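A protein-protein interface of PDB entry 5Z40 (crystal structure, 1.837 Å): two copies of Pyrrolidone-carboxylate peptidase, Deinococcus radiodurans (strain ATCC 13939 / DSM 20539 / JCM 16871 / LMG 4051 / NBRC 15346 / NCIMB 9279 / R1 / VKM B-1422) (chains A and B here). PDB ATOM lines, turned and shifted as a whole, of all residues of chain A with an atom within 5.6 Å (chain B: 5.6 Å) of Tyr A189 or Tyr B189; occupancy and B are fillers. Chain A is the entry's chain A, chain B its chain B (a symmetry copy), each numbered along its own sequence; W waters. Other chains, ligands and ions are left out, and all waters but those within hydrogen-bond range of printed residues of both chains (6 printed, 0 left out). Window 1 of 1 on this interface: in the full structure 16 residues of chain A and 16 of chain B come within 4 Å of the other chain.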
ATOM      1  N   ARG A  75     -11.101  10.001 -33.753  1.00  0.00           N
ATOM      2  CA  ARG A  75     -11.695   9.187 -32.699  1.00  0.00           C
ATOM      3  C   ARG A  75     -12.055  10.071 -31.511  1.00  0.00           C
ATOM      4  O   ARG A  75     -11.348  11.045 -31.223  1.00  0.00           O
ATOM      5  CB  ARG A  75     -10.758   8.060 -32.256  1.00  0.00           C
ATOM      6  CG  ARG A  75     -10.459   7.095 -33.352  1.00  0.00           C
ATOM      7  CD  ARG A  75      -9.688   5.897 -32.838  1.00  0.00           C
ATOM      8  NE  ARG A  75      -9.317   5.037 -33.964  1.00  0.00           N
ATOM      9  CZ  ARG A  75      -8.638   3.897 -33.847  1.00  0.00           C
ATOM     10  NH1 ARG A  75      -8.210   3.488 -32.658  1.00  0.00           N
ATOM     11  NH2 ARG A  75      -8.330   3.204 -34.944  1.00  0.00           N
ATOM     12  N   PRO A  76     -13.161   9.787 -30.831  1.00  0.00           N
ATOM     13  CA  PRO A  76     -13.609  10.670 -29.741  1.00  0.00           C
ATOM     14  C   PRO A  76     -12.992  10.339 -28.392  1.00  0.00           C
ATOM     15  O   PRO A  76     -13.003  11.187 -27.492  1.00  0.00           O
ATOM     16  CB  PRO A  76     -15.125  10.445 -29.709  1.00  0.00           C
ATOM     17  CG  PRO A  76     -15.291   9.013 -30.216  1.00  0.00           C
ATOM     18  CD  PRO A  76     -14.192   8.819 -31.245  1.00  0.00           C
ATOM     19  N   GLN A  77     -12.511   9.101 -28.229  1.00  0.00           N
ATOM     20  CA  GLN A  77     -12.059   8.591 -26.939  1.00  0.00           C
ATOM     21  C   GLN A  77     -10.782   7.793 -27.133  1.00  0.00           C
ATOM     22  O   GLN A  77     -10.544   7.223 -28.204  1.00  0.00           O
ATOM     23  CB  GLN A  77     -13.133   7.712 -26.244  1.00  0.00           C
ATOM     24  CG  GLN A  77     -14.469   8.455 -26.104  1.00  0.00           C
ATOM     25  CD  GLN A  77     -15.625   7.582 -25.607  1.00  0.00           C
ATOM     26  OE1 GLN A  77     -15.452   6.387 -25.389  1.00  0.00           O
ATOM     27  NE2 GLN A  77     -16.811   8.187 -25.447  1.00  0.00           N
ATOM     28  N   GLU A 130     -12.956   7.988 -14.487  1.00  0.00           N
ATOM     29  CA  GLU A 130     -13.958   8.732 -15.264  1.00  0.00           C
ATOM     30  C   GLU A 130     -13.494   9.039 -16.685  1.00  0.00           C
ATOM     31  O   GLU A 130     -13.885  10.071 -17.261  1.00  0.00           O
ATOM     32  CB  GLU A 130     -14.372  10.035 -14.573  1.00  0.00           C
ATOM     33  CG  GLU A 130     -15.016   9.847 -13.208  1.00  0.00           C
ATOM     34  CD  GLU A 130     -16.425   9.288 -13.327  1.00  0.00           C
ATOM     35  OE1 GLU A 130     -17.219   9.822 -14.143  1.00  0.00           O
ATOM     36  OE2 GLU A 130     -16.730   8.302 -12.620  1.00  0.00           O
ATOM     37  N   ILE A 131     -12.688   8.163 -17.276  1.00  0.00           N
ATOM     38  CA  ILE A 131     -12.214   8.349 -18.647  1.00  0.00           C
ATOM     39  C   ILE A 131     -12.936   7.360 -19.557  1.00  0.00           C
ATOM     40  O   ILE A 131     -12.784   6.136 -19.392  1.00  0.00           O
ATOM     41  CB  ILE A 131     -10.695   8.185 -18.768  1.00  0.00           C
ATOM     42  CG1 ILE A 131      -9.988   9.218 -17.869  1.00  0.00           C
ATOM     43  CG2 ILE A 131     -10.275   8.390 -20.218  1.00  0.00           C
ATOM     44  CD1 ILE A 131      -8.524   8.898 -17.587  1.00  0.00           C
ATOM     45  N   PRO A 132     -13.716   7.844 -20.515  1.00  0.00           N
ATOM     46  CA  PRO A 132     -14.322   6.953 -21.514  1.00  0.00           C
ATOM     47  C   PRO A 132     -13.253   6.344 -22.409  1.00  0.00           C
ATOM     48  O   PRO A 132     -12.298   7.014 -22.791  1.00  0.00           O
ATOM     49  CB  PRO A 132     -15.244   7.891 -22.315  1.00  0.00           C
ATOM     50  CG  PRO A 132     -15.420   9.120 -21.490  1.00  0.00           C
ATOM     51  CD  PRO A 132     -14.156   9.242 -20.664  1.00  0.00           C
ATOM     52  N   PRO A 171      -7.215  10.662 -29.112  1.00  0.00           N
ATOM     53  CA  PRO A 171      -7.843  11.696 -29.945  1.00  0.00           C
ATOM     54  C   PRO A 171      -6.927  12.881 -30.230  1.00  0.00           C
ATOM     55  O   PRO A 171      -5.879  13.103 -29.607  1.00  0.00           O
ATOM     56  CB  PRO A 171      -9.042  12.151 -29.099  1.00  0.00           C
ATOM     57  CG  PRO A 171      -9.368  10.960 -28.220  1.00  0.00           C
ATOM     58  CD  PRO A 171      -8.028  10.303 -27.931  1.00  0.00           C
ATOM     59  N   ALA A 172      -7.386  13.702 -31.179  1.00  0.00           N
ATOM     60  CA  ALA A 172      -6.820  15.040 -31.355  1.00  0.00           C
ATOM     61  C   ALA A 172      -6.821  15.805 -30.038  1.00  0.00           C
ATOM     62  O   ALA A 172      -7.722  15.643 -29.212  1.00  0.00           O
ATOM     63  CB  ALA A 172      -7.649  15.804 -32.388  1.00  0.00           C
ATOM     64  N   ASN A 173      -5.802  16.648 -29.820  1.00  0.00           N
ATOM     65  CA  ASN A 173      -5.889  17.622 -28.741  1.00  0.00           C
ATOM     66  C   ASN A 173      -6.468  18.907 -29.331  1.00  0.00           C
ATOM     67  O   ASN A 173      -6.925  18.921 -30.480  1.00  0.00           O
ATOM     68  CB  ASN A 173      -4.534  17.830 -28.056  1.00  0.00           C
ATOM     69  CG  ASN A 173      -3.447  18.299 -29.013  1.00  0.00           C
ATOM     70  OD1 ASN A 173      -3.719  18.658 -30.156  1.00  0.00           O
ATOM     71  ND2 ASN A 173      -2.203  18.261 -28.552  1.00  0.00           N
ATOM     72  N   ALA A 174      -6.448  20.001 -28.553  1.00  0.00           N
ATOM     73  CA  ALA A 174      -7.005  21.262 -29.035  1.00  0.00           C
ATOM     74  C   ALA A 174      -6.229  21.774 -30.245  1.00  0.00           C
ATOM     75  O   ALA A 174      -6.823  22.257 -31.219  1.00  0.00           O
ATOM     76  CB  ALA A 174      -7.010  22.302 -27.922  1.00  0.00           C
ATOM     77  N   ALA A 177      -7.276  19.950 -33.399  1.00  0.00           N
ATOM     78  CA  ALA A 177      -8.617  20.325 -33.834  1.00  0.00           C
ATOM     79  C   ALA A 177      -8.651  21.739 -34.401  1.00  0.00           C
ATOM     80  O   ALA A 177      -9.365  22.009 -35.374  1.00  0.00           O
ATOM     81  CB  ALA A 177      -9.595  20.209 -32.663  1.00  0.00           C
ATOM     82  N   LEU A 187     -13.271  18.060 -35.652  1.00  0.00           N
ATOM     83  CA  LEU A 187     -12.765  16.855 -35.016  1.00  0.00           C
ATOM     84  C   LEU A 187     -13.229  16.764 -33.567  1.00  0.00           C
ATOM     85  O   LEU A 187     -13.198  17.766 -32.832  1.00  0.00           O
ATOM     86  CB  LEU A 187     -11.241  16.836 -35.027  1.00  0.00           C
ATOM     87  CG  LEU A 187     -10.508  16.624 -36.346  1.00  0.00           C
ATOM     88  CD1 LEU A 187      -9.017  16.737 -36.077  1.00  0.00           C
ATOM     89  CD2 LEU A 187     -10.886  15.270 -36.923  1.00  0.00           C
ATOM     90  N   PRO A 188     -13.621  15.575 -33.125  1.00  0.00           N
ATOM     91  CA  PRO A 188     -13.603  15.314 -31.685  1.00  0.00           C
ATOM     92  C   PRO A 188     -12.193  15.566 -31.185  1.00  0.00           C
ATOM     93  O   PRO A 188     -11.215  15.337 -31.899  1.00  0.00           O
ATOM     94  CB  PRO A 188     -13.985  13.836 -31.577  1.00  0.00           C
ATOM     95  CG  PRO A 188     -14.727  13.536 -32.859  1.00  0.00           C
ATOM     96  CD  PRO A 188     -14.080  14.414 -33.906  1.00  0.00           C
ATOM     97  N   TYR A 189     -12.094  16.038 -29.948  1.00  0.00           N
ATOM     98  CA  TYR A 189     -10.799  16.361 -29.363  1.00  0.00           C
ATOM     99  C   TYR A 189     -10.888  16.202 -27.853  1.00  0.00           C
ATOM    100  O   TYR A 189     -11.975  16.105 -27.282  1.00  0.00           O
ATOM    101  CB  TYR A 189     -10.335  17.789 -29.727  1.00  0.00           C
ATOM    102  CG  TYR A 189     -10.966  18.923 -28.929  1.00  0.00           C
ATOM    103  CD1 TYR A 189     -12.237  19.408 -29.235  1.00  0.00           C
ATOM    104  CD2 TYR A 189     -10.260  19.543 -27.901  1.00  0.00           C
ATOM    105  CE1 TYR A 189     -12.811  20.457 -28.511  1.00  0.00           C
ATOM    106  CE2 TYR A 189     -10.823  20.590 -27.171  1.00  0.00           C
ATOM    107  CZ  TYR A 189     -12.099  21.027 -27.474  1.00  0.00           C
ATOM    108  OH  TYR A 189     -12.651  22.040 -26.767  1.00  0.00           O
ATOM    109  N   LEU A 190      -9.724  16.192 -27.209  1.00  0.00           N
ATOM    110  CA  LEU A 190      -9.625  16.264 -25.760  1.00  0.00           C
ATOM    111  C   LEU A 190      -8.527  17.248 -25.391  1.00  0.00           C
ATOM    112  O   LEU A 190      -7.532  17.363 -26.115  1.00  0.00           O
ATOM    113  CB  LEU A 190      -9.316  14.892 -25.144  1.00  0.00           C
ATOM    114  CG  LEU A 190     -10.427  13.862 -25.346  1.00  0.00           C
ATOM    115  CD1 LEU A 190      -9.958  12.480 -24.901  1.00  0.00           C
ATOM    116  CD2 LEU A 190     -11.692  14.279 -24.602  1.00  0.00           C
ATOM    117  N   PRO A 191      -8.691  17.994 -24.303  1.00  0.00           N
ATOM    118  CA  PRO A 191      -7.553  18.777 -23.796  1.00  0.00           C
ATOM    119  C   PRO A 191      -6.368  17.857 -23.570  1.00  0.00           C
ATOM    120  O   PRO A 191      -6.523  16.717 -23.130  1.00  0.00           O
ATOM    121  CB  PRO A 191      -8.069  19.369 -22.483  1.00  0.00           C
ATOM    122  CG  PRO A 191      -9.571  19.423 -22.662  1.00  0.00           C
ATOM    123  CD  PRO A 191      -9.925  18.237 -23.536  1.00  0.00           C
ATOM    124  N   GLU A 194      -6.229  15.902 -20.398  1.00  0.00           N
ATOM    125  CA  GLU A 194      -7.047  14.686 -20.392  1.00  0.00           C
ATOM    126  C   GLU A 194      -6.329  13.529 -21.081  1.00  0.00           C
ATOM    127  O   GLU A 194      -6.313  12.409 -20.567  1.00  0.00           O
ATOM    128  CB  GLU A 194      -8.385  14.969 -21.072  1.00  0.00           C
ATOM    129  CG  GLU A 194      -9.362  13.811 -21.198  1.00  0.00           C
ATOM    130  CD  GLU A 194     -10.012  13.341 -19.913  1.00  0.00           C
ATOM    131  OE1 GLU A 194     -10.940  12.524 -20.024  1.00  0.00           O
ATOM    132  OE2 GLU A 194      -9.624  13.756 -18.794  1.00  0.00           O
ATOM    133  N   ARG B  75     -22.199  16.334 -30.381  1.00  0.00           N
ATOM    134  CA  ARG B  75     -21.358  17.348 -31.002  1.00  0.00           C
ATOM    135  C   ARG B  75     -19.965  17.314 -30.378  1.00  0.00           C
ATOM    136  O   ARG B  75     -19.831  17.108 -29.165  1.00  0.00           O
ATOM    137  CB  ARG B  75     -21.966  18.747 -30.862  1.00  0.00           C
ATOM    138  CG  ARG B  75     -23.266  18.899 -31.568  1.00  0.00           C
ATOM    139  CD  ARG B  75     -23.758  20.331 -31.570  1.00  0.00           C
ATOM    140  NE  ARG B  75     -25.099  20.414 -32.159  1.00  0.00           N
ATOM    141  CZ  ARG B  75     -25.753  21.566 -32.328  1.00  0.00           C
ATOM    142  NH1 ARG B  75     -25.202  22.704 -31.924  1.00  0.00           N
ATOM    143  NH2 ARG B  75     -26.978  21.576 -32.844  1.00  0.00           N
ATOM    144  N   PRO B  76     -18.915  17.515 -31.174  1.00  0.00           N
ATOM    145  CA  PRO B  76     -17.542  17.384 -30.659  1.00  0.00           C
ATOM    146  C   PRO B  76     -17.008  18.655 -30.008  1.00  0.00           C
ATOM    147  O   PRO B  76     -16.052  18.564 -29.235  1.00  0.00           O
ATOM    148  CB  PRO B  76     -16.734  17.018 -31.910  1.00  0.00           C
ATOM    149  CG  PRO B  76     -17.507  17.645 -33.038  1.00  0.00           C
ATOM    150  CD  PRO B  76     -18.966  17.549 -32.647  1.00  0.00           C
ATOM    151  N   GLN B  77     -17.584  19.825 -30.328  1.00  0.00           N
ATOM    152  CA  GLN B  77     -17.049  21.118 -29.930  1.00  0.00           C
ATOM    153  C   GLN B  77     -18.207  22.017 -29.534  1.00  0.00           C
ATOM    154  O   GLN B  77     -19.307  21.894 -30.077  1.00  0.00           O
ATOM    155  CB  GLN B  77     -16.278  21.800 -31.052  1.00  0.00           C
ATOM    156  CG  GLN B  77     -15.128  20.954 -31.527  1.00  0.00           C
ATOM    157  CD  GLN B  77     -14.449  21.471 -32.791  1.00  0.00           C
ATOM    158  OE1 GLN B  77     -14.823  22.507 -33.323  1.00  0.00           O
ATOM    159  NE2 GLN B  77     -13.374  20.794 -33.201  1.00  0.00           N
ATOM    160  N   GLU B 130      -7.560  28.826 -27.253  1.00  0.00           N
ATOM    161  CA  GLU B 130      -7.285  27.474 -27.748  1.00  0.00           C
ATOM    162  C   GLU B 130      -8.492  26.548 -27.638  1.00  0.00           C
ATOM    163  O   GLU B 130      -8.313  25.335 -27.462  1.00  0.00           O
ATOM    164  CB  GLU B 130      -6.101  26.824 -27.019  1.00  0.00           C
ATOM    165  CG  GLU B 130      -4.789  27.566 -27.127  1.00  0.00           C
ATOM    166  CD  GLU B 130      -4.187  27.452 -28.505  1.00  0.00           C
ATOM    167  OE1 GLU B 130      -4.128  26.317 -29.049  1.00  0.00           O
ATOM    168  OE2 GLU B 130      -3.771  28.502 -29.045  1.00  0.00           O
ATOM    169  N   ILE B 131      -9.706  27.076 -27.769  1.00  0.00           N
ATOM    170  CA  ILE B 131     -10.926  26.267 -27.714  1.00  0.00           C
ATOM    171  C   ILE B 131     -11.517  26.163 -29.116  1.00  0.00           C
ATOM    172  O   ILE B 131     -11.921  27.188 -29.698  1.00  0.00           O
ATOM    173  CB  ILE B 131     -11.962  26.835 -26.730  1.00  0.00           C
ATOM    174  CG1 ILE B 131     -11.363  26.875 -25.316  1.00  0.00           C
ATOM    175  CG2 ILE B 131     -13.260  26.010 -26.776  1.00  0.00           C
ATOM    176  CD1 ILE B 131     -12.167  27.757 -24.370  1.00  0.00           C
ATOM    177  N   PRO B 132     -11.611  24.960 -29.680  1.00  0.00           N
ATOM    178  CA  PRO B 132     -12.315  24.787 -30.962  1.00  0.00           C
ATOM    179  C   PRO B 132     -13.801  25.069 -30.799  1.00  0.00           C
ATOM    180  O   PRO B 132     -14.402  24.721 -29.781  1.00  0.00           O
ATOM    181  CB  PRO B 132     -12.069  23.312 -31.311  1.00  0.00           C
ATOM    182  CG  PRO B 132     -10.964  22.853 -30.498  1.00  0.00           C
ATOM    183  CD  PRO B 132     -10.991  23.701 -29.219  1.00  0.00           C
ATOM    184  N   PRO B 171     -20.773  20.025 -25.694  1.00  0.00           N
ATOM    185  CA  PRO B 171     -20.660  18.562 -25.794  1.00  0.00           C
ATOM    186  C   PRO B 171     -20.998  17.839 -24.501  1.00  0.00           C
ATOM    187  O   PRO B 171     -21.043  18.404 -23.405  1.00  0.00           O
ATOM    188  CB  PRO B 171     -19.184  18.339 -26.150  1.00  0.00           C
ATOM    189  CG  PRO B 171     -18.766  19.629 -26.843  1.00  0.00           C
ATOM    190  CD  PRO B 171     -19.555  20.727 -26.145  1.00  0.00           C
ATOM    191  N   ALA B 172     -21.157  16.520 -24.646  1.00  0.00           N
ATOM    192  CA  ALA B 172     -21.168  15.631 -23.489  1.00  0.00           C
ATOM    193  C   ALA B 172     -19.937  15.902 -22.635  1.00  0.00           C
ATOM    194  O   ALA B 172     -18.875  16.217 -23.174  1.00  0.00           O
ATOM    195  CB  ALA B 172     -21.154  14.175 -23.960  1.00  0.00           C
ATOM    196  N   ASN B 173     -20.072  15.795 -21.298  1.00  0.00           N
ATOM    197  CA  ASN B 173     -18.885  15.713 -20.447  1.00  0.00           C
ATOM    198  C   ASN B 173     -18.543  14.228 -20.275  1.00  0.00           C
ATOM    199  O   ASN B 173     -19.147  13.364 -20.928  1.00  0.00           O
ATOM    200  CB  ASN B 173     -19.085  16.438 -19.105  1.00  0.00           C
ATOM    201  CG  ASN B 173     -20.265  15.895 -18.297  1.00  0.00           C
ATOM    202  OD1 ASN B 173     -20.849  14.878 -18.646  1.00  0.00           O
ATOM    203  ND2 ASN B 173     -20.580  16.556 -17.180  1.00  0.00           N
ATOM    204  N   ALA B 174     -17.594  13.910 -19.380  1.00  0.00           N
ATOM    205  CA  ALA B 174     -17.201  12.520 -19.167  1.00  0.00           C
ATOM    206  C   ALA B 174     -18.373  11.687 -18.648  1.00  0.00           C
ATOM    207  O   ALA B 174     -18.600  10.558 -19.108  1.00  0.00           O
ATOM    208  CB  ALA B 174     -16.029  12.441 -18.181  1.00  0.00           C
ATOM    209  N   ALA B 177     -20.744  10.732 -21.406  1.00  0.00           N
ATOM    210  CA  ALA B 177     -20.152   9.739 -22.302  1.00  0.00           C
ATOM    211  C   ALA B 177     -20.039   8.367 -21.640  1.00  0.00           C
ATOM    212  O   ALA B 177     -20.220   7.335 -22.305  1.00  0.00           O
ATOM    213  CB  ALA B 177     -18.776  10.220 -22.771  1.00  0.00           C
ATOM    214  N   LEU B 187     -19.560   8.654 -27.689  1.00  0.00           N
ATOM    215  CA  LEU B 187     -19.805  10.076 -27.876  1.00  0.00           C
ATOM    216  C   LEU B 187     -18.499  10.855 -27.844  1.00  0.00           C
ATOM    217  O   LEU B 187     -17.639  10.588 -27.000  1.00  0.00           O
ATOM    218  CB  LEU B 187     -20.710  10.624 -26.775  1.00  0.00           C
ATOM    219  CG  LEU B 187     -22.179  10.223 -26.741  1.00  0.00           C
ATOM    220  CD1 LEU B 187     -22.807  10.821 -25.486  1.00  0.00           C
ATOM    221  CD2 LEU B 187     -22.872  10.687 -27.995  1.00  0.00           C
ATOM    222  N   PRO B 188     -18.331  11.848 -28.712  1.00  0.00           N
ATOM    223  CA  PRO B 188     -17.344  12.888 -28.417  1.00  0.00           C
ATOM    224  C   PRO B 188     -17.690  13.513 -27.077  1.00  0.00           C
ATOM    225  O   PRO B 188     -18.857  13.596 -26.690  1.00  0.00           O
ATOM    226  CB  PRO B 188     -17.502  13.883 -29.571  1.00  0.00           C
ATOM    227  CG  PRO B 188     -18.073  13.093 -30.680  1.00  0.00           C
ATOM    228  CD  PRO B 188     -18.975  12.054 -30.022  1.00  0.00           C
ATOM    229  N   TYR B 189     -16.660  13.941 -26.356  1.00  0.00           N
ATOM    230  CA  TYR B 189     -16.897  14.520 -25.045  1.00  0.00           C
ATOM    231  C   TYR B 189     -15.785  15.504 -24.742  1.00  0.00           C
ATOM    232  O   TYR B 189     -14.769  15.547 -25.429  1.00  0.00           O
ATOM    233  CB  TYR B 189     -16.998  13.440 -23.951  1.00  0.00           C
ATOM    234  CG  TYR B 189     -15.668  12.877 -23.478  1.00  0.00           C
ATOM    235  CD1 TYR B 189     -15.004  11.898 -24.209  1.00  0.00           C
ATOM    236  CD2 TYR B 189     -15.092  13.318 -22.292  1.00  0.00           C
ATOM    237  CE1 TYR B 189     -13.784  11.381 -23.773  1.00  0.00           C
ATOM    238  CE2 TYR B 189     -13.889  12.807 -21.846  1.00  0.00           C
ATOM    239  CZ  TYR B 189     -13.240  11.848 -22.600  1.00  0.00           C
ATOM    240  OH  TYR B 189     -12.055  11.350 -22.160  1.00  0.00           O
ATOM    241  N   LEU B 190     -15.997  16.304 -23.706  1.00  0.00           N
ATOM    242  CA  LEU B 190     -14.960  17.168 -23.142  1.00  0.00           C
ATOM    243  C   LEU B 190     -15.024  17.061 -21.629  1.00  0.00           C
ATOM    244  O   LEU B 190     -16.104  16.858 -21.065  1.00  0.00           O
ATOM    245  CB  LEU B 190     -15.152  18.634 -23.559  1.00  0.00           C
ATOM    246  CG  LEU B 190     -15.008  18.905 -25.065  1.00  0.00           C
ATOM    247  CD1 LEU B 190     -15.407  20.310 -25.401  1.00  0.00           C
ATOM    248  CD2 LEU B 190     -13.588  18.580 -25.536  1.00  0.00           C
ATOM    249  N   PRO B 191     -13.870  17.138 -20.947  1.00  0.00           N
ATOM    250  CA  PRO B 191     -13.886  17.292 -19.487  1.00  0.00           C
ATOM    251  C   PRO B 191     -14.731  18.496 -19.116  1.00  0.00           C
ATOM    252  O   PRO B 191     -14.697  19.535 -19.781  1.00  0.00           O
ATOM    253  CB  PRO B 191     -12.411  17.508 -19.136  1.00  0.00           C
ATOM    254  CG  PRO B 191     -11.638  16.848 -20.255  1.00  0.00           C
ATOM    255  CD  PRO B 191     -12.500  17.033 -21.477  1.00  0.00           C
ATOM    256  N   GLU B 194     -13.122  21.860 -19.275  1.00  0.00           N
ATOM    257  CA  GLU B 194     -13.052  22.469 -20.608  1.00  0.00           C
ATOM    258  C   GLU B 194     -14.381  23.118 -20.992  1.00  0.00           C
ATOM    259  O   GLU B 194     -14.406  24.240 -21.504  1.00  0.00           O
ATOM    260  CB  GLU B 194     -12.648  21.413 -21.638  1.00  0.00           C
ATOM    261  CG  GLU B 194     -12.632  21.864 -23.111  1.00  0.00           C
ATOM    262  CD  GLU B 194     -11.466  22.744 -23.485  1.00  0.00           C
ATOM    263  OE1 GLU B 194     -10.713  23.192 -22.584  1.00  0.00           O
ATOM    264  OE2 GLU B 194     -11.297  22.982 -24.702  1.00  0.00           O
HETATM  265  O   HOH W   1     -11.825  20.806 -35.745  1.00  0.00           O
HETATM  266  O   HOH W   2     -11.186   9.221 -23.851  1.00  0.00           O
HETATM  267  O   HOH W   3     -14.213  13.450 -27.730  1.00  0.00           O
HETATM  268  O   HOH W   4     -19.560   7.160 -24.987  1.00  0.00           O
HETATM  269  O   HOH W   5     -15.016  22.839 -27.983  1.00  0.00           O
HETATM  270  O   HOH W   6     -14.783  16.385 -28.832  1.00  0.00           O
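Pro A76 touches Tyr B189, and with the chains exchanged Tyr A189 touches Pro B76. Gln A77 touches Leu B187, and with the chains exchanged Leu A187 touches Gln B77. Glu A130 touches Ala B174, and with the chains exchanged Ala A174 touches Glu B130. Pro A132 touches Ala B177, and with the chains exchanged Ala A177 touches Pro B132. 17 positions are printed for both chains.
Among the printed residues, 27 pairs touch across the chains.
Pro A76 touches Leu B187 (CB to O, 3.7 Å). Tyr B189 touches Pro A76. Gln A77 touches Tyr B189 (CG to CE1, 3.8 Å). OH of Tyr B189 touches CD of Pro A132 (3.3 Å). Pro B76 touches Pro A188 (CB to CA, 3.6 Å). Pro B76 touches Tyr A189 (O to CE1, 3.8 Å). Gln B77 touches Tyr A189 (CG to CE1, 3.8 Å). Tyr A189 touches Pro B132. O of Tyr A189 touches CD2 of Leu B190, at 3.4 Å. Pro B191 touches Glu A194 (CG to CB, 3.8 Å).
Water W6 bridges O of Pro B76 and N of Tyr A189. Water W3 lies within hydrogen-bond range of the backbone carbonyl oxygen (O) of Pro A76 (2.6 Å) and the backbone NH (N) of Tyr B189 (2.8 Å). Water W5 lies within hydrogen-bond range of O of Pro B132 (2.7 Å) and OH of Tyr A189 (2.8 Å). Water W2 bridges O of Pro A132 and OH of Tyr B189. Water W1 lies within hydrogen-bond range of the backbone carbonyl oxygen of Ala A177 (2.8 Å), the side-chain amide nitrogen of Gln B77 (3.0 Å) and the backbone NH of Leu A187 (3.1 Å). Water W4 lies within hydrogen-bond range of the backbone carbonyl oxygen of Ala B177 (2.8 Å), the side-chain amide nitrogen of Gln A77 (3.0 Å) and the backbone NH of Leu B187 (3.1 Å).
The backbone NH (N) of Leu A190 is in hydrogen-bond range of the backbone carbonyl oxygen (O) of Ala A172 (2.9 Å). O of Ala B172 lies within hydrogen-bond range of N of Leu B190, 2.9 Å away.
Of the printed residues of chain B, Pro A76 touches Leu B187, Pro B188 and Tyr B189. Of the printed residues of chain B, Tyr A189 touches Pro B76 (3.8 Å), Gln B77 (3.8 Å), Pro B132 (3.4 Å), Tyr B189 (3.4 Å), Leu B190 (3.4 Å) and Glu B194 (2.6 Å). Asn B173 touches none of the printed residues of chain A. Printed residues of chain A within 4 Å of Glu B194: Tyr A189 and Pro A191. The nearest printed residue of chain B that does not touch Tyr A189 is Ile B131 (4.02 Å). The nearest residue of chain A that does not touch Tyr B189 is Glu A130 (5.3 Å).
NE2 of Gln A77 lies within hydrogen-bond range of O of Leu B187, at 3.0 Å. The side-chain carboxylate (OE2) of Glu B194 is in hydrogen-bond range of the side-chain hydroxyl (OH) of Tyr A189. The side-chain carboxylate (OE1) of Glu A194 sits at hydrogen-bond distance from the side-chain hydroxyl (OH) of Tyr B189 (2.7 Å). The backbone carbonyl oxygen (O) of Leu A187 is in hydrogen-bond range of the side-chain amide nitrogen (NE2) of Gln B77 (3.1 Å). O of Tyr A189 lies close to O of Tyr B189, 3.4 Å away.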
